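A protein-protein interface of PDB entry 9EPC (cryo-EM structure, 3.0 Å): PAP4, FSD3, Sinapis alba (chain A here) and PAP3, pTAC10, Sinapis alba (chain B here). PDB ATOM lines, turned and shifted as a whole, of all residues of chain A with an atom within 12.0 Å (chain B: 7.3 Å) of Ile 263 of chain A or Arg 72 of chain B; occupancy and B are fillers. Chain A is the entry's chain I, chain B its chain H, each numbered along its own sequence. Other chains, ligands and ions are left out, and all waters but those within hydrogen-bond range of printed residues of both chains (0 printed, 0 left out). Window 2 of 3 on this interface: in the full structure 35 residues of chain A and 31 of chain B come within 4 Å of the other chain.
NH2 of Arg 73 of chain B is in salt-bridge range of OE2 of Glu 258 of chain A. The side-chain amide oxygen (OD1) of Asn 260 of chain A sits at hydrogen-bond distance from the indole nitrogen (NE1) of Trp 312 of chain B. The guanidinium group (NH2) of Arg 72 of chain B lies close to the backbone carbonyl oxygen (O) of Ile 263 of chain A (3.1 Å).
The side-chain carboxylate (OD1) of Asp 69 of chain B is in salt-bridge range of the guanidinium group (NH1) of Arg 72 of chain B, at 3.6 Å. O of Asn 75 of chain B sits at hydrogen-bond distance from N of Trp 81 of chain B. The guanidinium group of Arg 72 of chain B is in hydrogen-bond range of the backbone carbonyl oxygen of Glu 68 of chain B (3.4 Å).
Among the printed residues, pairs that only touch across the chains: Pro 259 of chain A with Trp 76 of chain B (3.8 Å), Ile 261 of chain A with Arg 73 of chain B (3.7 Å), Ile 261 of chain A with Trp 76 of chain B (3.3 Å), Pro 262 of chain A with Arg 72 of chain B (3.4 Å), Pro 262 of chain A with Trp 76 of chain B (3.4 Å), Pro 262 of chain A with Trp 312 of chain B (3.5 Å) and Ala 264 of chain A with Trp 81 of chain B (3.5 Å).
Printed residues of chain A within 4 Å of Arg 72 of chain B: Pro 262 (3.4 Å) and Ile 263 (3.1 Å). Glu 68 of chain B touches none of the printed residues of chain A. No residue of chain A comes within 4 Å of Ala 71 of chain B. Arg 73 of chain B touches just these residues of chain A: Glu 258 (2.7 Å) and Ile 261 (3.7 Å). No residue of chain A comes within 4 Å of Asn 75 of chain B. Of the printed residues of chain A, Trp 81 of chain B touches Ala 264. Of the printed residues of chain B, Ala 264 of chain A touches Trp 81. Of the printed residues of chain A, Trp 312 of chain B touches Asn 260 and Pro 262. Printed residues of chain B within 4 Å of Ile 261 of chain A: Arg 73 and Trp 76. Of the printed residues of chain B, Asn 260 of chain A touches Trp 312. Of the printed residues of chain B, Pro 262 of chain A touches Arg 72 (3.4 Å), Trp 76 (3.4 Å) and Trp 312 (3.5 Å). The nearest printed residue of chain A that does not touch Arg 72 of chain B is Ile 261 of chain A (4.01 Å). The nearest printed residue of chain B that does not touch Ala 264 of chain A is Pro 83 of chain B (4.1 Å).
Of the 17 printed residues of chain B, 5 touch a printed residue of chain A. Hydrophobic or aromatic side chains of chain B within 4 Å of the printed part of chain A: Trp 76, Trp 81 and Trp 312. Along chain B the printed residues that touch a printed residue of chain A span positions 72 to 312. Hydrophobic or aromatic side chains of chain A that line the printed part of chain B: Pro 259, Ile 261, Pro 262 and Ile 263. Among the printed residues, 10 pairs touch across the chains.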
ATOM      1  N   GLU A 258     -15.755  12.731  22.968  1.00  0.00           N
ATOM      2  CA  GLU A 258     -16.698  13.822  22.795  1.00  0.00           C
ATOM      3  C   GLU A 258     -16.655  14.298  21.350  1.00  0.00           C
ATOM      4  O   GLU A 258     -15.574  14.371  20.753  1.00  0.00           O
ATOM      5  CB  GLU A 258     -16.362  14.978  23.752  1.00  0.00           C
ATOM      6  CG  GLU A 258     -17.418  16.065  23.852  1.00  0.00           C
ATOM      7  CD  GLU A 258     -17.121  17.256  22.962  1.00  0.00           C
ATOM      8  OE1 GLU A 258     -15.928  17.522  22.704  1.00  0.00           O
ATOM      9  OE2 GLU A 258     -18.077  17.925  22.517  1.00  0.00           O
ATOM     10  N   PRO A 259     -17.806  14.622  20.755  1.00  0.00           N
ATOM     11  CA  PRO A 259     -17.818  15.016  19.338  1.00  0.00           C
ATOM     12  C   PRO A 259     -17.129  16.345  19.066  1.00  0.00           C
ATOM     13  O   PRO A 259     -16.604  16.990  19.977  1.00  0.00           O
ATOM     14  CB  PRO A 259     -19.315  15.086  19.008  1.00  0.00           C
ATOM     15  CG  PRO A 259     -19.991  15.258  20.320  1.00  0.00           C
ATOM     16  CD  PRO A 259     -19.168  14.486  21.296  1.00  0.00           C
ATOM     17  N   ASN A 260     -17.129  16.756  17.802  1.00  0.00           N
ATOM     18  CA  ASN A 260     -16.402  17.924  17.316  1.00  0.00           C
ATOM     19  C   ASN A 260     -17.340  18.856  16.565  1.00  0.00           C
ATOM     20  O   ASN A 260     -17.112  19.208  15.406  1.00  0.00           O
ATOM     21  CB  ASN A 260     -15.222  17.509  16.445  1.00  0.00           C
ATOM     22  CG  ASN A 260     -15.599  16.476  15.414  1.00  0.00           C
ATOM     23  OD1 ASN A 260     -16.486  15.655  15.641  1.00  0.00           O
ATOM     24  ND2 ASN A 260     -14.927  16.507  14.269  1.00  0.00           N
ATOM     25  N   ILE A 261     -18.436  19.227  17.224  1.00  0.00           N
ATOM     26  CA  ILE A 261     -19.525  20.040  16.681  1.00  0.00           C
ATOM     27  C   ILE A 261     -19.005  21.147  15.770  1.00  0.00           C
ATOM     28  O   ILE A 261     -18.208  21.987  16.207  1.00  0.00           O
ATOM     29  CB  ILE A 261     -20.363  20.656  17.811  1.00  0.00           C
ATOM     30  CG1 ILE A 261     -20.352  19.759  19.050  1.00  0.00           C
ATOM     31  CG2 ILE A 261     -21.782  20.913  17.344  1.00  0.00           C
ATOM     32  CD1 ILE A 261     -21.066  18.455  18.872  1.00  0.00           C
ATOM     33  N   PRO A 262     -19.418  21.177  14.505  1.00  0.00           N
ATOM     34  CA  PRO A 262     -18.987  22.255  13.611  1.00  0.00           C
ATOM     35  C   PRO A 262     -19.525  23.599  14.067  1.00  0.00           C
ATOM     36  O   PRO A 262     -20.591  23.694  14.677  1.00  0.00           O
ATOM     37  CB  PRO A 262     -19.578  21.853  12.255  1.00  0.00           C
ATOM     38  CG  PRO A 262     -19.897  20.408  12.382  1.00  0.00           C
ATOM     39  CD  PRO A 262     -20.252  20.188  13.812  1.00  0.00           C
ATOM     40  N   ILE A 263     -18.764  24.652  13.766  1.00  0.00           N
ATOM     41  CA  ILE A 263     -19.173  25.995  14.160  1.00  0.00           C
ATOM     42  C   ILE A 263     -20.389  26.443  13.360  1.00  0.00           C
ATOM     43  O   ILE A 263     -21.299  27.085  13.898  1.00  0.00           O
ATOM     44  CB  ILE A 263     -17.996  26.974  14.009  1.00  0.00           C
ATOM     45  CG1 ILE A 263     -16.784  26.465  14.788  1.00  0.00           C
ATOM     46  CG2 ILE A 263     -18.390  28.356  14.495  1.00  0.00           C
ATOM     47  CD1 ILE A 263     -17.034  26.306  16.272  1.00  0.00           C
ATOM     48  N   ALA A 264     -20.429  26.115  12.073  1.00  0.00           N
ATOM     49  CA  ALA A 264     -21.548  26.501  11.220  1.00  0.00           C
ATOM     50  C   ALA A 264     -22.826  25.777  11.628  1.00  0.00           C
ATOM     51  O   ALA A 264     -23.608  26.286  12.431  1.00  0.00           O
ATOM     52  CB  ALA A 264     -21.224  26.218   9.764  1.00  0.00           C
ATOM     53  N   ASP B  66     -28.606  29.825  27.742  1.00  0.00           N
ATOM     54  CA  ASP B  66     -27.712  28.990  26.948  1.00  0.00           C
ATOM     55  C   ASP B  66     -27.132  29.840  25.830  1.00  0.00           C
ATOM     56  O   ASP B  66     -27.883  30.383  25.015  1.00  0.00           O
ATOM     57  CB  ASP B  66     -28.445  27.776  26.375  1.00  0.00           C
ATOM     58  CG  ASP B  66     -28.168  26.506  27.153  1.00  0.00           C
ATOM     59  OD1 ASP B  66     -27.349  26.550  28.095  1.00  0.00           O
ATOM     60  OD2 ASP B  66     -28.766  25.461  26.821  1.00  0.00           O
ATOM     61  N   THR B  67     -25.809  29.956  25.795  1.00  0.00           N
ATOM     62  CA  THR B  67     -25.157  30.714  24.742  1.00  0.00           C
ATOM     63  C   THR B  67     -25.268  29.972  23.413  1.00  0.00           C
ATOM     64  O   THR B  67     -25.676  28.809  23.349  1.00  0.00           O
ATOM     65  CB  THR B  67     -23.689  30.959  25.087  1.00  0.00           C
ATOM     66  OG1 THR B  67     -23.002  29.705  25.170  1.00  0.00           O
ATOM     67  CG2 THR B  67     -23.573  31.679  26.417  1.00  0.00           C
ATOM     68  N   GLU B  68     -24.894  30.658  22.334  1.00  0.00           N
ATOM     69  CA  GLU B  68     -24.905  30.015  21.027  1.00  0.00           C
ATOM     70  C   GLU B  68     -23.620  29.217  20.838  1.00  0.00           C
ATOM     71  O   GLU B  68     -22.970  29.294  19.791  1.00  0.00           O
ATOM     72  CB  GLU B  68     -25.069  31.067  19.925  1.00  0.00           C
ATOM     73  CG  GLU B  68     -25.493  30.525  18.568  1.00  0.00           C
ATOM     74  CD  GLU B  68     -26.954  30.137  18.517  1.00  0.00           C
ATOM     75  OE1 GLU B  68     -27.682  30.396  19.498  1.00  0.00           O
ATOM     76  OE2 GLU B  68     -27.376  29.573  17.489  1.00  0.00           O
ATOM     77  N   ASP B  69     -23.249  28.452  21.862  1.00  0.00           N
ATOM     78  CA  ASP B  69     -22.205  27.438  21.764  1.00  0.00           C
ATOM     79  C   ASP B  69     -22.557  26.148  22.477  1.00  0.00           C
ATOM     80  O   ASP B  69     -22.002  25.102  22.127  1.00  0.00           O
ATOM     81  CB  ASP B  69     -20.880  27.969  22.321  1.00  0.00           C
ATOM     82  CG  ASP B  69     -20.234  28.991  21.412  1.00  0.00           C
ATOM     83  OD1 ASP B  69     -20.223  28.770  20.184  1.00  0.00           O
ATOM     84  OD2 ASP B  69     -19.739  30.015  21.924  1.00  0.00           O
ATOM     85  N   GLU B  70     -23.450  26.179  23.462  1.00  0.00           N
ATOM     86  CA  GLU B  70     -23.920  24.989  24.151  1.00  0.00           C
ATOM     87  C   GLU B  70     -25.287  24.537  23.669  1.00  0.00           C
ATOM     88  O   GLU B  70     -25.560  23.333  23.654  1.00  0.00           O
ATOM     89  CB  GLU B  70     -23.966  25.245  25.660  1.00  0.00           C
ATOM     90  CG  GLU B  70     -24.582  26.584  26.025  1.00  0.00           C
ATOM     91  CD  GLU B  70     -24.278  27.000  27.449  1.00  0.00           C
ATOM     92  OE1 GLU B  70     -23.691  26.188  28.195  1.00  0.00           O
ATOM     93  OE2 GLU B  70     -24.624  28.140  27.821  1.00  0.00           O
ATOM     94  N   ALA B  71     -26.150  25.476  23.279  1.00  0.00           N
ATOM     95  CA  ALA B  71     -27.389  25.103  22.607  1.00  0.00           C
ATOM     96  C   ALA B  71     -27.096  24.420  21.280  1.00  0.00           C
ATOM     97  O   ALA B  71     -27.761  23.445  20.913  1.00  0.00           O
ATOM     98  CB  ALA B  71     -28.268  26.334  22.399  1.00  0.00           C
ATOM     99  N   ARG B  72     -26.104  24.924  20.543  1.00  0.00           N
ATOM    100  CA  ARG B  72     -25.655  24.234  19.340  1.00  0.00           C
ATOM    101  C   ARG B  72     -25.123  22.849  19.672  1.00  0.00           C
ATOM    102  O   ARG B  72     -25.441  21.871  18.985  1.00  0.00           O
ATOM    103  CB  ARG B  72     -24.582  25.058  18.634  1.00  0.00           C
ATOM    104  CG  ARG B  72     -23.885  24.320  17.511  1.00  0.00           C
ATOM    105  CD  ARG B  72     -22.524  24.923  17.240  1.00  0.00           C
ATOM    106  NE  ARG B  72     -22.614  26.349  16.965  1.00  0.00           N
ATOM    107  CZ  ARG B  72     -21.576  27.173  16.944  1.00  0.00           C
ATOM    108  NH1 ARG B  72     -20.350  26.744  17.195  1.00  0.00           N
ATOM    109  NH2 ARG B  72     -21.774  28.458  16.667  1.00  0.00           N
ATOM    110  N   ARG B  73     -24.311  22.746  20.725  1.00  0.00           N
ATOM    111  CA  ARG B  73     -23.833  21.439  21.163  1.00  0.00           C
ATOM    112  C   ARG B  73     -24.988  20.559  21.616  1.00  0.00           C
ATOM    113  O   ARG B  73     -25.016  19.358  21.326  1.00  0.00           O
ATOM    114  CB  ARG B  73     -22.807  21.604  22.282  1.00  0.00           C
ATOM    115  CG  ARG B  73     -22.647  20.378  23.163  1.00  0.00           C
ATOM    116  CD  ARG B  73     -21.400  20.464  24.025  1.00  0.00           C
ATOM    117  NE  ARG B  73     -20.195  20.139  23.273  1.00  0.00           N
ATOM    118  CZ  ARG B  73     -19.408  21.032  22.689  1.00  0.00           C
ATOM    119  NH1 ARG B  73     -19.661  22.328  22.760  1.00  0.00           N
ATOM    120  NH2 ARG B  73     -18.338  20.613  22.018  1.00  0.00           N
ATOM    121  N   ARG B  74     -25.955  21.140  22.328  1.00  0.00           N
ATOM    122  CA  ARG B  74     -27.119  20.372  22.753  1.00  0.00           C
ATOM    123  C   ARG B  74     -27.910  19.867  21.555  1.00  0.00           C
ATOM    124  O   ARG B  74     -28.405  18.734  21.562  1.00  0.00           O
ATOM    125  CB  ARG B  74     -28.004  21.221  23.660  1.00  0.00           C
ATOM    126  CG  ARG B  74     -29.188  20.474  24.240  1.00  0.00           C
ATOM    127  CD  ARG B  74     -30.036  21.391  25.098  1.00  0.00           C
ATOM    128  NE  ARG B  74     -29.212  22.213  25.973  1.00  0.00           N
ATOM    129  CZ  ARG B  74     -28.743  21.820  27.148  1.00  0.00           C
ATOM    130  NH1 ARG B  74     -29.004  20.615  27.628  1.00  0.00           N
ATOM    131  NH2 ARG B  74     -27.990  22.655  27.860  1.00  0.00           N
ATOM    132  N   ASN B  75     -28.043  20.695  20.517  1.00  0.00           N
ATOM    133  CA  ASN B  75     -28.763  20.269  19.323  1.00  0.00           C
ATOM    134  C   ASN B  75     -28.072  19.091  18.650  1.00  0.00           C
ATOM    135  O   ASN B  75     -28.732  18.144  18.210  1.00  0.00           O
ATOM    136  CB  ASN B  75     -28.902  21.433  18.345  1.00  0.00           C
ATOM    137  CG  ASN B  75     -29.898  22.467  18.812  1.00  0.00           C
ATOM    138  OD1 ASN B  75     -30.743  22.194  19.661  1.00  0.00           O
ATOM    139  ND2 ASN B  75     -29.812  23.664  18.249  1.00  0.00           N
ATOM    140  N   TRP B  76     -26.744  19.132  18.555  1.00  0.00           N
ATOM    141  CA  TRP B  76     -26.020  18.019  17.950  1.00  0.00           C
ATOM    142  C   TRP B  76     -26.189  16.744  18.767  1.00  0.00           C
ATOM    143  O   TRP B  76     -26.437  15.667  18.214  1.00  0.00           O
ATOM    144  CB  TRP B  76     -24.541  18.370  17.802  1.00  0.00           C
ATOM    145  CG  TRP B  76     -23.712  17.266  17.213  1.00  0.00           C
ATOM    146  CD1 TRP B  76     -23.306  16.123  17.837  1.00  0.00           C
ATOM    147  CD2 TRP B  76     -23.169  17.213  15.891  1.00  0.00           C
ATOM    148  NE1 TRP B  76     -22.558  15.357  16.983  1.00  0.00           N
ATOM    149  CE2 TRP B  76     -22.457  16.004  15.781  1.00  0.00           C
ATOM    150  CE3 TRP B  76     -23.220  18.065  14.787  1.00  0.00           C
ATOM    151  CZ2 TRP B  76     -21.803  15.629  14.615  1.00  0.00           C
ATOM    152  CZ3 TRP B  76     -22.573  17.689  13.630  1.00  0.00           C
ATOM    153  CH2 TRP B  76     -21.872  16.483  13.553  1.00  0.00           C
ATOM    154  N   ILE B  77     -26.056  16.846  20.088  1.00  0.00           N
ATOM    155  CA  ILE B  77     -26.031  15.648  20.920  1.00  0.00           C
ATOM    156  C   ILE B  77     -27.439  15.104  21.125  1.00  0.00           C
ATOM    157  O   ILE B  77     -27.689  13.906  20.955  1.00  0.00           O
ATOM    158  CB  ILE B  77     -25.338  15.941  22.260  1.00  0.00           C
ATOM    159  CG1 ILE B  77     -23.891  16.368  22.023  1.00  0.00           C
ATOM    160  CG2 ILE B  77     -25.381  14.719  23.155  1.00  0.00           C
ATOM    161  CD1 ILE B  77     -23.139  16.680  23.289  1.00  0.00           C
ATOM    162  N   GLU B  78     -28.380  15.972  21.489  1.00  0.00           N
ATOM    163  CA  GLU B  78     -29.732  15.541  21.822  1.00  0.00           C
ATOM    164  C   GLU B  78     -30.681  15.599  20.631  1.00  0.00           C
ATOM    165  O   GLU B  78     -31.393  14.629  20.359  1.00  0.00           O
ATOM    166  CB  GLU B  78     -30.284  16.389  22.972  1.00  0.00           C
ATOM    167  CG  GLU B  78     -29.474  16.285  24.249  1.00  0.00           C
ATOM    168  CD  GLU B  78     -30.126  17.004  25.412  1.00  0.00           C
ATOM    169  OE1 GLU B  78     -31.213  17.587  25.219  1.00  0.00           O
ATOM    170  OE2 GLU B  78     -29.552  16.984  26.520  1.00  0.00           O
ATOM    171  N   TRP B  81     -28.657  17.397  15.552  1.00  0.00           N
ATOM    172  CA  TRP B  81     -28.452  18.428  14.548  1.00  0.00           C
ATOM    173  C   TRP B  81     -27.162  18.185  13.777  1.00  0.00           C
ATOM    174  O   TRP B  81     -26.214  17.581  14.282  1.00  0.00           O
ATOM    175  CB  TRP B  81     -28.418  19.807  15.206  1.00  0.00           C
ATOM    176  CG  TRP B  81     -28.010  20.907  14.286  1.00  0.00           C
ATOM    177  CD1 TRP B  81     -28.797  21.553  13.386  1.00  0.00           C
ATOM    178  CD2 TRP B  81     -26.709  21.493  14.174  1.00  0.00           C
ATOM    179  NE1 TRP B  81     -28.071  22.505  12.718  1.00  0.00           N
ATOM    180  CE2 TRP B  81     -26.785  22.488  13.184  1.00  0.00           C
ATOM    181  CE3 TRP B  81     -25.488  21.273  14.814  1.00  0.00           C
ATOM    182  CZ2 TRP B  81     -25.689  23.261  12.820  1.00  0.00           C
ATOM    183  CZ3 TRP B  81     -24.403  22.040  14.451  1.00  0.00           C
ATOM    184  CH2 TRP B  81     -24.510  23.022  13.464  1.00  0.00           C
ATOM    185  N   PRO B  83     -25.096  20.459  10.315  1.00  0.00           N
ATOM    186  CA  PRO B  83     -25.210  21.458   9.235  1.00  0.00           C
ATOM    187  C   PRO B  83     -25.023  20.831   7.859  1.00  0.00           C
ATOM    188  O   PRO B  83     -24.024  21.036   7.163  1.00  0.00           O
ATOM    189  CB  PRO B  83     -24.098  22.449   9.591  1.00  0.00           C
ATOM    190  CG  PRO B  83     -23.070  21.609  10.245  1.00  0.00           C
ATOM    191  CD  PRO B  83     -23.809  20.555  11.021  1.00  0.00           C
ATOM    192  N   ASP B 148     -14.985  22.530   7.094  1.00  0.00           N
ATOM    193  CA  ASP B 148     -13.705  21.931   7.439  1.00  0.00           C
ATOM    194  C   ASP B 148     -13.788  20.412   7.384  1.00  0.00           C
ATOM    195  O   ASP B 148     -14.758  19.807   7.846  1.00  0.00           O
ATOM    196  CB  ASP B 148     -13.276  22.383   8.833  1.00  0.00           C
ATOM    197  CG  ASP B 148     -14.337  22.118   9.881  1.00  0.00           C
ATOM    198  OD1 ASP B 148     -15.536  22.200   9.543  1.00  0.00           O
ATOM    199  OD2 ASP B 148     -13.975  21.824  11.038  1.00  0.00           O
ATOM    200  N   TRP B 312     -19.324  13.345   9.698  1.00  0.00           N
ATOM    201  CA  TRP B 312     -17.887  13.158   9.551  1.00  0.00           C
ATOM    202  C   TRP B 312     -17.527  11.819   8.930  1.00  0.00           C
ATOM    203  O   TRP B 312     -16.538  11.727   8.200  1.00  0.00           O
ATOM    204  CB  TRP B 312     -17.194  13.283  10.909  1.00  0.00           C
ATOM    205  CG  TRP B 312     -17.445  14.582  11.593  1.00  0.00           C
ATOM    206  CD1 TRP B 312     -18.122  14.776  12.758  1.00  0.00           C
ATOM    207  CD2 TRP B 312     -17.029  15.878  11.150  1.00  0.00           C
ATOM    208  NE1 TRP B 312     -18.149  16.110  13.073  1.00  0.00           N
ATOM    209  CE2 TRP B 312     -17.484  16.809  12.101  1.00  0.00           C
ATOM    210  CE3 TRP B 312     -16.314  16.340  10.044  1.00  0.00           C
ATOM    211  CZ2 TRP B 312     -17.248  18.172  11.979  1.00  0.00           C
ATOM    212  CZ3 TRP B 312     -16.081  17.693   9.925  1.00  0.00           C
ATOM    213  CH2 TRP B 312     -16.547  18.594  10.886  1.00  0.00           C
